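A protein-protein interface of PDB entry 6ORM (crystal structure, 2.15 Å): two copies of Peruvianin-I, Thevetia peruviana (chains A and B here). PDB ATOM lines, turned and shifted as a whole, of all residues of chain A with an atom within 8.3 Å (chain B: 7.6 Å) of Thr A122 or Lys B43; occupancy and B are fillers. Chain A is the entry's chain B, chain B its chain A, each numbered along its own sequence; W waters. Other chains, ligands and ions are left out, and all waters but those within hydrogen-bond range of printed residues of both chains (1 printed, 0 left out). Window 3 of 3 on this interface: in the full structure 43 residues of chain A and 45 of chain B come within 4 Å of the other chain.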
ATOM      1  N   VAL A  97     -11.030   6.471   9.996  1.00  0.00           N
ATOM      2  CA  VAL A  97     -10.112   6.442  11.126  1.00  0.00           C
ATOM      3  C   VAL A  97      -9.383   5.107  11.149  1.00  0.00           C
ATOM      4  O   VAL A  97     -10.012   4.047  11.049  1.00  0.00           O
ATOM      5  CB  VAL A  97     -10.870   6.675  12.442  1.00  0.00           C
ATOM      6  CG1 VAL A  97      -9.968   6.402  13.636  1.00  0.00           C
ATOM      7  CG2 VAL A  97     -11.440   8.090  12.489  1.00  0.00           C
ATOM      8  N   MET A  98      -8.059   5.149  11.283  1.00  0.00           N
ATOM      9  CA  MET A  98      -7.262   3.953  11.530  1.00  0.00           C
ATOM     10  C   MET A  98      -6.564   4.090  12.872  1.00  0.00           C
ATOM     11  O   MET A  98      -5.749   4.999  13.060  1.00  0.00           O
ATOM     12  CB  MET A  98      -6.220   3.710  10.436  1.00  0.00           C
ATOM     13  CG  MET A  98      -5.394   2.450  10.702  1.00  0.00           C
ATOM     14  SD  MET A  98      -4.376   1.904   9.319  1.00  0.00           S
ATOM     15  CE  MET A  98      -3.225   3.270   9.182  1.00  0.00           C
ATOM     16  N   ALA A  99      -6.873   3.184  13.793  1.00  0.00           N
ATOM     17  CA  ALA A  99      -6.155   3.119  15.055  1.00  0.00           C
ATOM     18  C   ALA A  99      -4.822   2.422  14.825  1.00  0.00           C
ATOM     19  O   ALA A  99      -4.761   1.388  14.154  1.00  0.00           O
ATOM     20  CB  ALA A  99      -6.976   2.376  16.108  1.00  0.00           C
ATOM     21  N   THR A 100      -3.751   2.994  15.374  1.00  0.00           N
ATOM     22  CA  THR A 100      -2.417   2.436  15.216  1.00  0.00           C
ATOM     23  C   THR A 100      -1.716   2.143  16.531  1.00  0.00           C
ATOM     24  O   THR A 100      -0.780   1.337  16.542  1.00  0.00           O
ATOM     25  CB  THR A 100      -1.532   3.384  14.390  1.00  0.00           C
ATOM     26  OG1 THR A 100      -1.470   4.662  15.035  1.00  0.00           O
ATOM     27  CG2 THR A 100      -2.100   3.556  12.989  1.00  0.00           C
ATOM     28  N   GLU A 101      -2.137   2.762  17.630  1.00  0.00           N
ATOM     29  CA  GLU A 101      -1.535   2.521  18.932  1.00  0.00           C
ATOM     30  C   GLU A 101      -2.601   2.692  20.002  1.00  0.00           C
ATOM     31  O   GLU A 101      -3.429   3.603  19.917  1.00  0.00           O
ATOM     32  CB  GLU A 101      -0.360   3.472  19.188  1.00  0.00           C
ATOM     33  CG  GLU A 101       0.228   3.374  20.585  1.00  0.00           C
ATOM     34  CD  GLU A 101       0.927   4.652  21.012  1.00  0.00           C
ATOM     35  OE1 GLU A 101       0.313   5.736  20.890  1.00  0.00           O
ATOM     36  OE2 GLU A 101       2.086   4.572  21.471  1.00  0.00           O
ATOM     37  N   GLY A 102      -2.573   1.818  21.001  1.00  0.00           N
ATOM     38  CA  GLY A 102      -3.523   1.895  22.093  1.00  0.00           C
ATOM     39  C   GLY A 102      -4.904   1.397  21.699  1.00  0.00           C
ATOM     40  O   GLY A 102      -5.081   0.685  20.706  1.00  0.00           O
ATOM     41  N   GLU A 103      -5.906   1.788  22.497  1.00  0.00           N
ATOM     42  CA  GLU A 103      -7.289   1.356  22.305  1.00  0.00           C
ATOM     43  C   GLU A 103      -8.236   2.504  22.580  1.00  0.00           C
ATOM     44  O   GLU A 103      -8.084   3.229  23.572  1.00  0.00           O
ATOM     45  CB  GLU A 103      -7.683   0.176  23.212  1.00  0.00           C
ATOM     46  CG  GLU A 103      -6.634  -0.908  23.261  1.00  0.00           C
ATOM     47  CD  GLU A 103      -5.663  -0.703  24.423  1.00  0.00           C
ATOM     48  OE1 GLU A 103      -4.449  -0.502  24.203  1.00  0.00           O
ATOM     49  OE2 GLU A 103      -6.154  -0.781  25.561  1.00  0.00           O
ATOM     50  N   ILE A 104      -9.234   2.643  21.710  1.00  0.00           N
ATOM     51  CA  ILE A 104     -10.148   3.773  21.746  1.00  0.00           C
ATOM     52  C   ILE A 104     -11.583   3.300  21.587  1.00  0.00           C
ATOM     53  O   ILE A 104     -11.853   2.242  21.012  1.00  0.00           O
ATOM     54  CB  ILE A 104      -9.830   4.814  20.653  1.00  0.00           C
ATOM     55  CG1 ILE A 104      -9.824   4.147  19.273  1.00  0.00           C
ATOM     56  CG2 ILE A 104      -8.523   5.512  20.938  1.00  0.00           C
ATOM     57  CD1 ILE A 104      -9.580   5.109  18.127  1.00  0.00           C
ATOM     58  N   LEU A 105     -12.504   4.099  22.117  1.00  0.00           N
ATOM     59  CA  LEU A 105     -13.909   4.050  21.743  1.00  0.00           C
ATOM     60  C   LEU A 105     -14.161   5.108  20.677  1.00  0.00           C
ATOM     61  O   LEU A 105     -13.905   6.294  20.905  1.00  0.00           O
ATOM     62  CB  LEU A 105     -14.813   4.292  22.951  1.00  0.00           C
ATOM     63  CG  LEU A 105     -15.082   3.116  23.887  1.00  0.00           C
ATOM     64  CD1 LEU A 105     -16.158   3.489  24.893  1.00  0.00           C
ATOM     65  CD2 LEU A 105     -15.487   1.882  23.093  1.00  0.00           C
ATOM     66  N   LYS A 119     -17.819   1.654  18.522  1.00  0.00           N
ATOM     67  CA  LYS A 119     -17.045   0.424  18.565  1.00  0.00           C
ATOM     68  C   LYS A 119     -15.705   0.681  19.234  1.00  0.00           C
ATOM     69  O   LYS A 119     -15.164   1.790  19.187  1.00  0.00           O
ATOM     70  CB  LYS A 119     -16.810  -0.165  17.163  1.00  0.00           C
ATOM     71  CG  LYS A 119     -18.039  -0.804  16.532  1.00  0.00           C
ATOM     72  CD  LYS A 119     -18.535  -1.994  17.345  1.00  0.00           C
ATOM     73  CE  LYS A 119     -17.526  -3.134  17.365  1.00  0.00           C
ATOM     74  NZ  LYS A 119     -18.056  -4.324  18.098  1.00  0.00           N
ATOM     75  N   ARG A 120     -15.181  -0.369  19.857  1.00  0.00           N
ATOM     76  CA  ARG A 120     -13.825  -0.358  20.382  1.00  0.00           C
ATOM     77  C   ARG A 120     -12.846  -0.652  19.254  1.00  0.00           C
ATOM     78  O   ARG A 120     -13.024  -1.616  18.500  1.00  0.00           O
ATOM     79  CB  ARG A 120     -13.687  -1.404  21.487  1.00  0.00           C
ATOM     80  CG  ARG A 120     -12.383  -1.357  22.245  1.00  0.00           C
ATOM     81  CD  ARG A 120     -12.326  -2.491  23.250  1.00  0.00           C
ATOM     82  NE  ARG A 120     -11.165  -2.367  24.123  1.00  0.00           N
ATOM     83  CZ  ARG A 120     -11.199  -1.809  25.327  1.00  0.00           C
ATOM     84  NH1 ARG A 120     -12.339  -1.319  25.804  1.00  0.00           N
ATOM     85  NH2 ARG A 120     -10.093  -1.737  26.052  1.00  0.00           N
ATOM     86  N   LEU A 121     -11.823   0.190  19.125  1.00  0.00           N
ATOM     87  CA  LEU A 121     -10.800   0.026  18.104  1.00  0.00           C
ATOM     88  C   LEU A 121      -9.461  -0.276  18.764  1.00  0.00           C
ATOM     89  O   LEU A 121      -9.082   0.367  19.747  1.00  0.00           O
ATOM     90  CB  LEU A 121     -10.670   1.278  17.229  1.00  0.00           C
ATOM     91  CG  LEU A 121     -11.917   1.891  16.587  1.00  0.00           C
ATOM     92  CD1 LEU A 121     -11.518   3.018  15.642  1.00  0.00           C
ATOM     93  CD2 LEU A 121     -12.724   0.839  15.853  1.00  0.00           C
ATOM     94  N   THR A 122      -8.752  -1.258  18.218  1.00  0.00           N
ATOM     95  CA  THR A 122      -7.387  -1.575  18.618  1.00  0.00           C
ATOM     96  C   THR A 122      -6.508  -1.446  17.373  1.00  0.00           C
ATOM     97  O   THR A 122      -7.054  -1.300  16.272  1.00  0.00           O
ATOM     98  CB  THR A 122      -7.332  -2.969  19.259  1.00  0.00           C
ATOM     99  OG1 THR A 122      -7.593  -3.965  18.270  1.00  0.00           O
ATOM    100  CG2 THR A 122      -8.366  -3.090  20.379  1.00  0.00           C
ATOM    101  N   PRO A 123      -5.175  -1.462  17.486  1.00  0.00           N
ATOM    102  CA  PRO A 123      -4.330  -1.179  16.313  1.00  0.00           C
ATOM    103  C   PRO A 123      -4.666  -2.051  15.110  1.00  0.00           C
ATOM    104  O   PRO A 123      -4.784  -3.275  15.214  1.00  0.00           O
ATOM    105  CB  PRO A 123      -2.917  -1.458  16.829  1.00  0.00           C
ATOM    106  CG  PRO A 123      -2.999  -1.173  18.279  1.00  0.00           C
ATOM    107  CD  PRO A 123      -4.354  -1.657  18.698  1.00  0.00           C
ATOM    108  N   GLY A 124      -4.802  -1.403  13.950  1.00  0.00           N
ATOM    109  CA  GLY A 124      -5.185  -2.047  12.718  1.00  0.00           C
ATOM    110  C   GLY A 124      -6.630  -1.809  12.320  1.00  0.00           C
ATOM    111  O   GLY A 124      -6.951  -1.866  11.127  1.00  0.00           O
ATOM    112  N   ASP A 125      -7.502  -1.548  13.290  1.00  0.00           N
ATOM    113  CA  ASP A 125      -8.919  -1.368  13.008  1.00  0.00           C
ATOM    114  C   ASP A 125      -9.180  -0.068  12.257  1.00  0.00           C
ATOM    115  O   ASP A 125      -8.493   0.940  12.447  1.00  0.00           O
ATOM    116  CB  ASP A 125      -9.731  -1.368  14.302  1.00  0.00           C
ATOM    117  CG  ASP A 125      -9.851  -2.742  14.911  1.00  0.00           C
ATOM    118  OD1 ASP A 125      -9.794  -3.733  14.153  1.00  0.00           O
ATOM    119  OD2 ASP A 125     -10.002  -2.838  16.146  1.00  0.00           O
ATOM    120  N   LEU A 126     -10.209  -0.100  11.414  1.00  0.00           N
ATOM    121  CA  LEU A 126     -10.703   1.069  10.708  1.00  0.00           C
ATOM    122  C   LEU A 126     -12.129   1.363  11.147  1.00  0.00           C
ATOM    123  O   LEU A 126     -12.884   0.455  11.507  1.00  0.00           O
ATOM    124  CB  LEU A 126     -10.677   0.870   9.194  1.00  0.00           C
ATOM    125  CG  LEU A 126      -9.344   0.489   8.563  1.00  0.00           C
ATOM    126  CD1 LEU A 126      -9.584   0.061   7.136  1.00  0.00           C
ATOM    127  CD2 LEU A 126      -8.381   1.653   8.621  1.00  0.00           C
ATOM    128  N   VAL A 140      -9.515   4.441  25.915  1.00  0.00           N
ATOM    129  CA  VAL A 140      -9.904   3.448  26.909  1.00  0.00           C
ATOM    130  C   VAL A 140      -8.760   2.494  27.212  1.00  0.00           C
ATOM    131  O   VAL A 140      -8.941   1.528  27.962  1.00  0.00           O
ATOM    132  CB  VAL A 140     -11.161   2.676  26.475  1.00  0.00           C
ATOM    133  CG1 VAL A 140     -12.341   3.625  26.338  1.00  0.00           C
ATOM    134  CG2 VAL A 140     -10.909   1.927  25.174  1.00  0.00           C
ATOM    135  N   THR A 146      -3.073   6.422  19.487  1.00  0.00           N
ATOM    136  CA  THR A 146      -2.780   7.127  18.248  1.00  0.00           C
ATOM    137  C   THR A 146      -3.693   6.592  17.158  1.00  0.00           C
ATOM    138  O   THR A 146      -3.830   5.375  16.999  1.00  0.00           O
ATOM    139  CB  THR A 146      -1.313   6.960  17.839  1.00  0.00           C
ATOM    140  OG1 THR A 146      -0.468   7.485  18.869  1.00  0.00           O
ATOM    141  CG2 THR A 146      -1.032   7.695  16.537  1.00  0.00           C
ATOM    142  N   PHE A 147      -4.323   7.500  16.421  1.00  0.00           N
ATOM    143  CA  PHE A 147      -5.083   7.119  15.244  1.00  0.00           C
ATOM    144  C   PHE A 147      -4.942   8.199  14.186  1.00  0.00           C
ATOM    145  O   PHE A 147      -4.662   9.362  14.492  1.00  0.00           O
ATOM    146  CB  PHE A 147      -6.566   6.846  15.567  1.00  0.00           C
ATOM    147  CG  PHE A 147      -7.301   8.005  16.191  1.00  0.00           C
ATOM    148  CD1 PHE A 147      -7.244   8.228  17.557  1.00  0.00           C
ATOM    149  CD2 PHE A 147      -8.095   8.838  15.418  1.00  0.00           C
ATOM    150  CE1 PHE A 147      -7.939   9.277  18.135  1.00  0.00           C
ATOM    151  CE2 PHE A 147      -8.793   9.888  15.992  1.00  0.00           C
ATOM    152  CZ  PHE A 147      -8.717  10.103  17.352  1.00  0.00           C
ATOM    153  N   ILE B  38     -16.969  -0.770  11.667  1.00  0.00           N
ATOM    154  CA  ILE B  38     -15.590  -1.139  11.948  1.00  0.00           C
ATOM    155  C   ILE B  38     -15.141  -2.135  10.885  1.00  0.00           C
ATOM    156  O   ILE B  38     -15.939  -2.930  10.376  1.00  0.00           O
ATOM    157  CB  ILE B  38     -15.447  -1.726  13.370  1.00  0.00           C
ATOM    158  CG1 ILE B  38     -13.976  -1.966  13.723  1.00  0.00           C
ATOM    159  CG2 ILE B  38     -16.253  -3.006  13.507  1.00  0.00           C
ATOM    160  CD1 ILE B  38     -13.770  -2.520  15.119  1.00  0.00           C
ATOM    161  N   TYR B  39     -13.863  -2.066  10.520  1.00  0.00           N
ATOM    162  CA  TYR B  39     -13.256  -3.069   9.653  1.00  0.00           C
ATOM    163  C   TYR B  39     -11.907  -3.460  10.233  1.00  0.00           C
ATOM    164  O   TYR B  39     -11.072  -2.592  10.504  1.00  0.00           O
ATOM    165  CB  TYR B  39     -13.088  -2.562   8.216  1.00  0.00           C
ATOM    166  CG  TYR B  39     -12.552  -3.623   7.278  1.00  0.00           C
ATOM    167  CD1 TYR B  39     -13.378  -4.636   6.805  1.00  0.00           C
ATOM    168  CD2 TYR B  39     -11.220  -3.620   6.881  1.00  0.00           C
ATOM    169  CE1 TYR B  39     -12.895  -5.612   5.955  1.00  0.00           C
ATOM    170  CE2 TYR B  39     -10.728  -4.592   6.031  1.00  0.00           C
ATOM    171  CZ  TYR B  39     -11.569  -5.586   5.572  1.00  0.00           C
ATOM    172  OH  TYR B  39     -11.088  -6.558   4.725  1.00  0.00           O
ATOM    173  N   SER B  40     -11.693  -4.765  10.415  1.00  0.00           N
ATOM    174  CA  SER B  40     -10.534  -5.272  11.141  1.00  0.00           C
ATOM    175  C   SER B  40      -9.607  -6.095  10.251  1.00  0.00           C
ATOM    176  O   SER B  40      -8.771  -6.847  10.763  1.00  0.00           O
ATOM    177  CB  SER B  40     -10.987  -6.106  12.342  1.00  0.00           C
ATOM    178  OG  SER B  40     -11.611  -5.294  13.320  1.00  0.00           O
ATOM    179  N   GLY B  41      -9.739  -5.966   8.929  1.00  0.00           N
ATOM    180  CA  GLY B  41      -8.946  -6.780   8.023  1.00  0.00           C
ATOM    181  C   GLY B  41      -7.447  -6.614   8.183  1.00  0.00           C
ATOM    182  O   GLY B  41      -6.690  -7.560   7.947  1.00  0.00           O
ATOM    183  N   PHE B  42      -6.992  -5.427   8.589  1.00  0.00           N
ATOM    184  CA  PHE B  42      -5.555  -5.199   8.706  1.00  0.00           C
ATOM    185  C   PHE B  42      -4.918  -5.998   9.831  1.00  0.00           C
ATOM    186  O   PHE B  42      -3.687  -6.075   9.891  1.00  0.00           O
ATOM    187  CB  PHE B  42      -5.258  -3.713   8.931  1.00  0.00           C
ATOM    188  CG  PHE B  42      -5.422  -2.867   7.706  1.00  0.00           C
ATOM    189  CD1 PHE B  42      -5.378  -3.431   6.443  1.00  0.00           C
ATOM    190  CD2 PHE B  42      -5.611  -1.501   7.820  1.00  0.00           C
ATOM    191  CE1 PHE B  42      -5.526  -2.647   5.315  1.00  0.00           C
ATOM    192  CE2 PHE B  42      -5.760  -0.710   6.698  1.00  0.00           C
ATOM    193  CZ  PHE B  42      -5.716  -1.283   5.443  1.00  0.00           C
ATOM    194  N   LYS B  43      -5.719  -6.600  10.711  1.00  0.00           N
ATOM    195  CA  LYS B  43      -5.163  -7.462  11.746  1.00  0.00           C
ATOM    196  C   LYS B  43      -4.624  -8.762  11.180  1.00  0.00           C
ATOM    197  O   LYS B  43      -3.833  -9.436  11.854  1.00  0.00           O
ATOM    198  CB  LYS B  43      -6.211  -7.737  12.820  1.00  0.00           C
ATOM    199  CG  LYS B  43      -6.493  -6.519  13.662  1.00  0.00           C
ATOM    200  CD  LYS B  43      -7.084  -6.898  14.989  1.00  0.00           C
ATOM    201  CE  LYS B  43      -7.274  -5.668  15.832  1.00  0.00           C
ATOM    202  NZ  LYS B  43      -8.703  -5.284  15.899  1.00  0.00           N
ATOM    203  N   GLN B  44      -5.038  -9.145   9.977  1.00  0.00           N
ATOM    204  CA  GLN B  44      -4.417 -10.264   9.290  1.00  0.00           C
ATOM    205  C   GLN B  44      -3.180  -9.772   8.565  1.00  0.00           C
ATOM    206  O   GLN B  44      -3.265  -8.864   7.718  1.00  0.00           O
ATOM    207  CB  GLN B  44      -5.415 -10.911   8.340  1.00  0.00           C
ATOM    208  CG  GLN B  44      -6.813 -10.964   8.932  1.00  0.00           C
ATOM    209  CD  GLN B  44      -7.855 -11.492   7.970  1.00  0.00           C
ATOM    210  OE1 GLN B  44      -7.528 -12.046   6.920  1.00  0.00           O
ATOM    211  NE2 GLN B  44      -9.128 -11.303   8.317  1.00  0.00           N
ATOM    212  N   ALA B  45      -2.032 -10.367   8.885  1.00  0.00           N
ATOM    213  CA  ALA B  45      -0.789 -10.076   8.200  1.00  0.00           C
ATOM    214  C   ALA B  45      -0.898 -10.469   6.730  1.00  0.00           C
ATOM    215  O   ALA B  45      -1.783 -11.240   6.351  1.00  0.00           O
ATOM    216  CB  ALA B  45       0.367 -10.817   8.870  1.00  0.00           C
ATOM    217  N   PRO B  46      -0.035  -9.920   5.877  1.00  0.00           N
ATOM    218  CA  PRO B  46       0.013 -10.390   4.489  1.00  0.00           C
ATOM    219  C   PRO B  46       0.133 -11.906   4.437  1.00  0.00           C
ATOM    220  O   PRO B  46       0.993 -12.501   5.089  1.00  0.00           O
ATOM    221  CB  PRO B  46       1.268  -9.704   3.936  1.00  0.00           C
ATOM    222  CG  PRO B  46       1.354  -8.441   4.719  1.00  0.00           C
ATOM    223  CD  PRO B  46       0.915  -8.814   6.111  1.00  0.00           C
ATOM    224  N   THR B  57      -3.270  -5.355   0.861  1.00  0.00           N
ATOM    225  CA  THR B  57      -4.494  -5.692   1.580  1.00  0.00           C
ATOM    226  C   THR B  57      -5.477  -4.554   1.325  1.00  0.00           C
ATOM    227  O   THR B  57      -5.260  -3.426   1.780  1.00  0.00           O
ATOM    228  CB  THR B  57      -4.228  -5.895   3.070  1.00  0.00           C
ATOM    229  OG1 THR B  57      -3.218  -6.897   3.238  1.00  0.00           O
ATOM    230  CG2 THR B  57      -5.499  -6.346   3.783  1.00  0.00           C
ATOM    231  N   ARG B  76      -3.315  -1.193   2.501  1.00  0.00           N
ATOM    232  CA  ARG B  76      -2.021  -1.449   3.119  1.00  0.00           C
ATOM    233  C   ARG B  76      -1.129  -2.179   2.129  1.00  0.00           C
ATOM    234  O   ARG B  76      -1.532  -3.196   1.556  1.00  0.00           O
ATOM    235  CB  ARG B  76      -2.161  -2.275   4.399  1.00  0.00           C
ATOM    236  CG  ARG B  76      -0.826  -2.519   5.096  1.00  0.00           C
ATOM    237  CD  ARG B  76      -0.935  -3.542   6.220  1.00  0.00           C
ATOM    238  NE  ARG B  76      -1.312  -4.864   5.732  1.00  0.00           N
ATOM    239  CZ  ARG B  76      -1.855  -5.815   6.487  1.00  0.00           C
ATOM    240  NH1 ARG B  76      -2.057  -5.606   7.781  1.00  0.00           N
ATOM    241  NH2 ARG B  76      -2.169  -6.988   5.953  1.00  0.00           N
HETATM  242  O   HOH W   1      -8.508  -3.230   9.346  1.00  0.00           O
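The backbone carbonyl oxygen (O) of Tyr B39 sits at hydrogen-bond distance from the backbone NH (N) of Leu A126. The side-chain hydroxyl (OG) of Ser B40 lies within hydrogen-bond range of the side-chain carboxylate (OD1) of Asp A125. The side-chain hydroxyl (OG1) of Thr A122 is in hydrogen-bond range of the side-chain amino group (NZ) of Lys B43 (2.9 Å). The side-chain carboxylate of Asp A125 is in salt-bridge range of the side-chain amino group of Lys B43 (2.6 Å).
The backbone carbonyl oxygen of Phe B42 sits at hydrogen-bond distance from the guanidinium group of Arg B76. N of Gly A124 lies within hydrogen-bond range of O of Ala A99. The backbone NH of Ala A99 lies within hydrogen-bond range of the backbone carbonyl oxygen of Asp A125, 3.1 Å away. The backbone NH (N) of Leu A121 sits at hydrogen-bond distance from the backbone carbonyl oxygen (O) of Ile A104 (2.8 Å). N of Thr A122 is in hydrogen-bond range of OD2 of Asp A125, 2.9 Å away.
Met A98 touches Phe B42. Arg A120 touches Ile B38 (O to CD1, 3.6 Å). CD1 of Ile B38 touches CD2 of Leu A121, 3.6 Å away. Lys B43 touches Pro A123 (CE to O, 3.5 Å). Phe B42 touches Gly A124 (CB to O, 3.3 Å). Asp A125 touches Ile B38 (OD2 to CD1, 3.9 Å). CA of Asp A125 touches O of Tyr B39, 3.5 Å away. Leu A126 touches Ile B38 (O to CA, 3.2 Å). Leu A126 touches Phe B42 (CD1 to CE2, 3.9 Å).
Ile A104 touches none of the printed residues of chain B. Of the printed residues of chain B, Leu A121 touches Ile B38 (3.6 Å). Thr A122 touches just one residue of chain B: Lys B43. Of the printed residues of chain B, Gly A124 touches Phe B42 (3.3 Å). Printed residues of chain B within 4 Å of Leu A126: Ile B38 (3.2 Å), Tyr B39 (2.8 Å) and Phe B42 (3.9 Å). Printed residues of chain A within 4 Å of Tyr B39: Asp A125 and Leu A126. Of the printed residues of chain A, Phe B42 touches Met A98 (3.9 Å), Gly A124 (3.3 Å) and Leu A126 (3.9 Å). Lys B43 touches three residues of chain A. The nearest printed residue of chain B that does not touch Pro A123 is Phe B42 (6.0 Å).
Hydrophobic or aromatic side chains of chain A within 4 Å of the printed part of chain B: Met A98, Leu A121 and Leu A126. Printed residues of chain B that touch a printed residue of chain A: Ile B38, Tyr B39, Ser B40, Phe B42 and Lys B43. Along chain B the printed residues that touch a printed residue of chain A span positions 38 to 43. Among the printed residues, 13 pairs touch across the chains.
No position is printed for both chains. Of the 13 pairs that touch across the chains among the printed residues, none has its exchanged pair printed and touching as well.
Water W1 lies within hydrogen-bond range of O of Gly A124 (2.7 Å), N of Phe B42 (2.8 Å), O of Tyr B39 (2.9 Å) and N of Gly B41 (3.0 Å).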
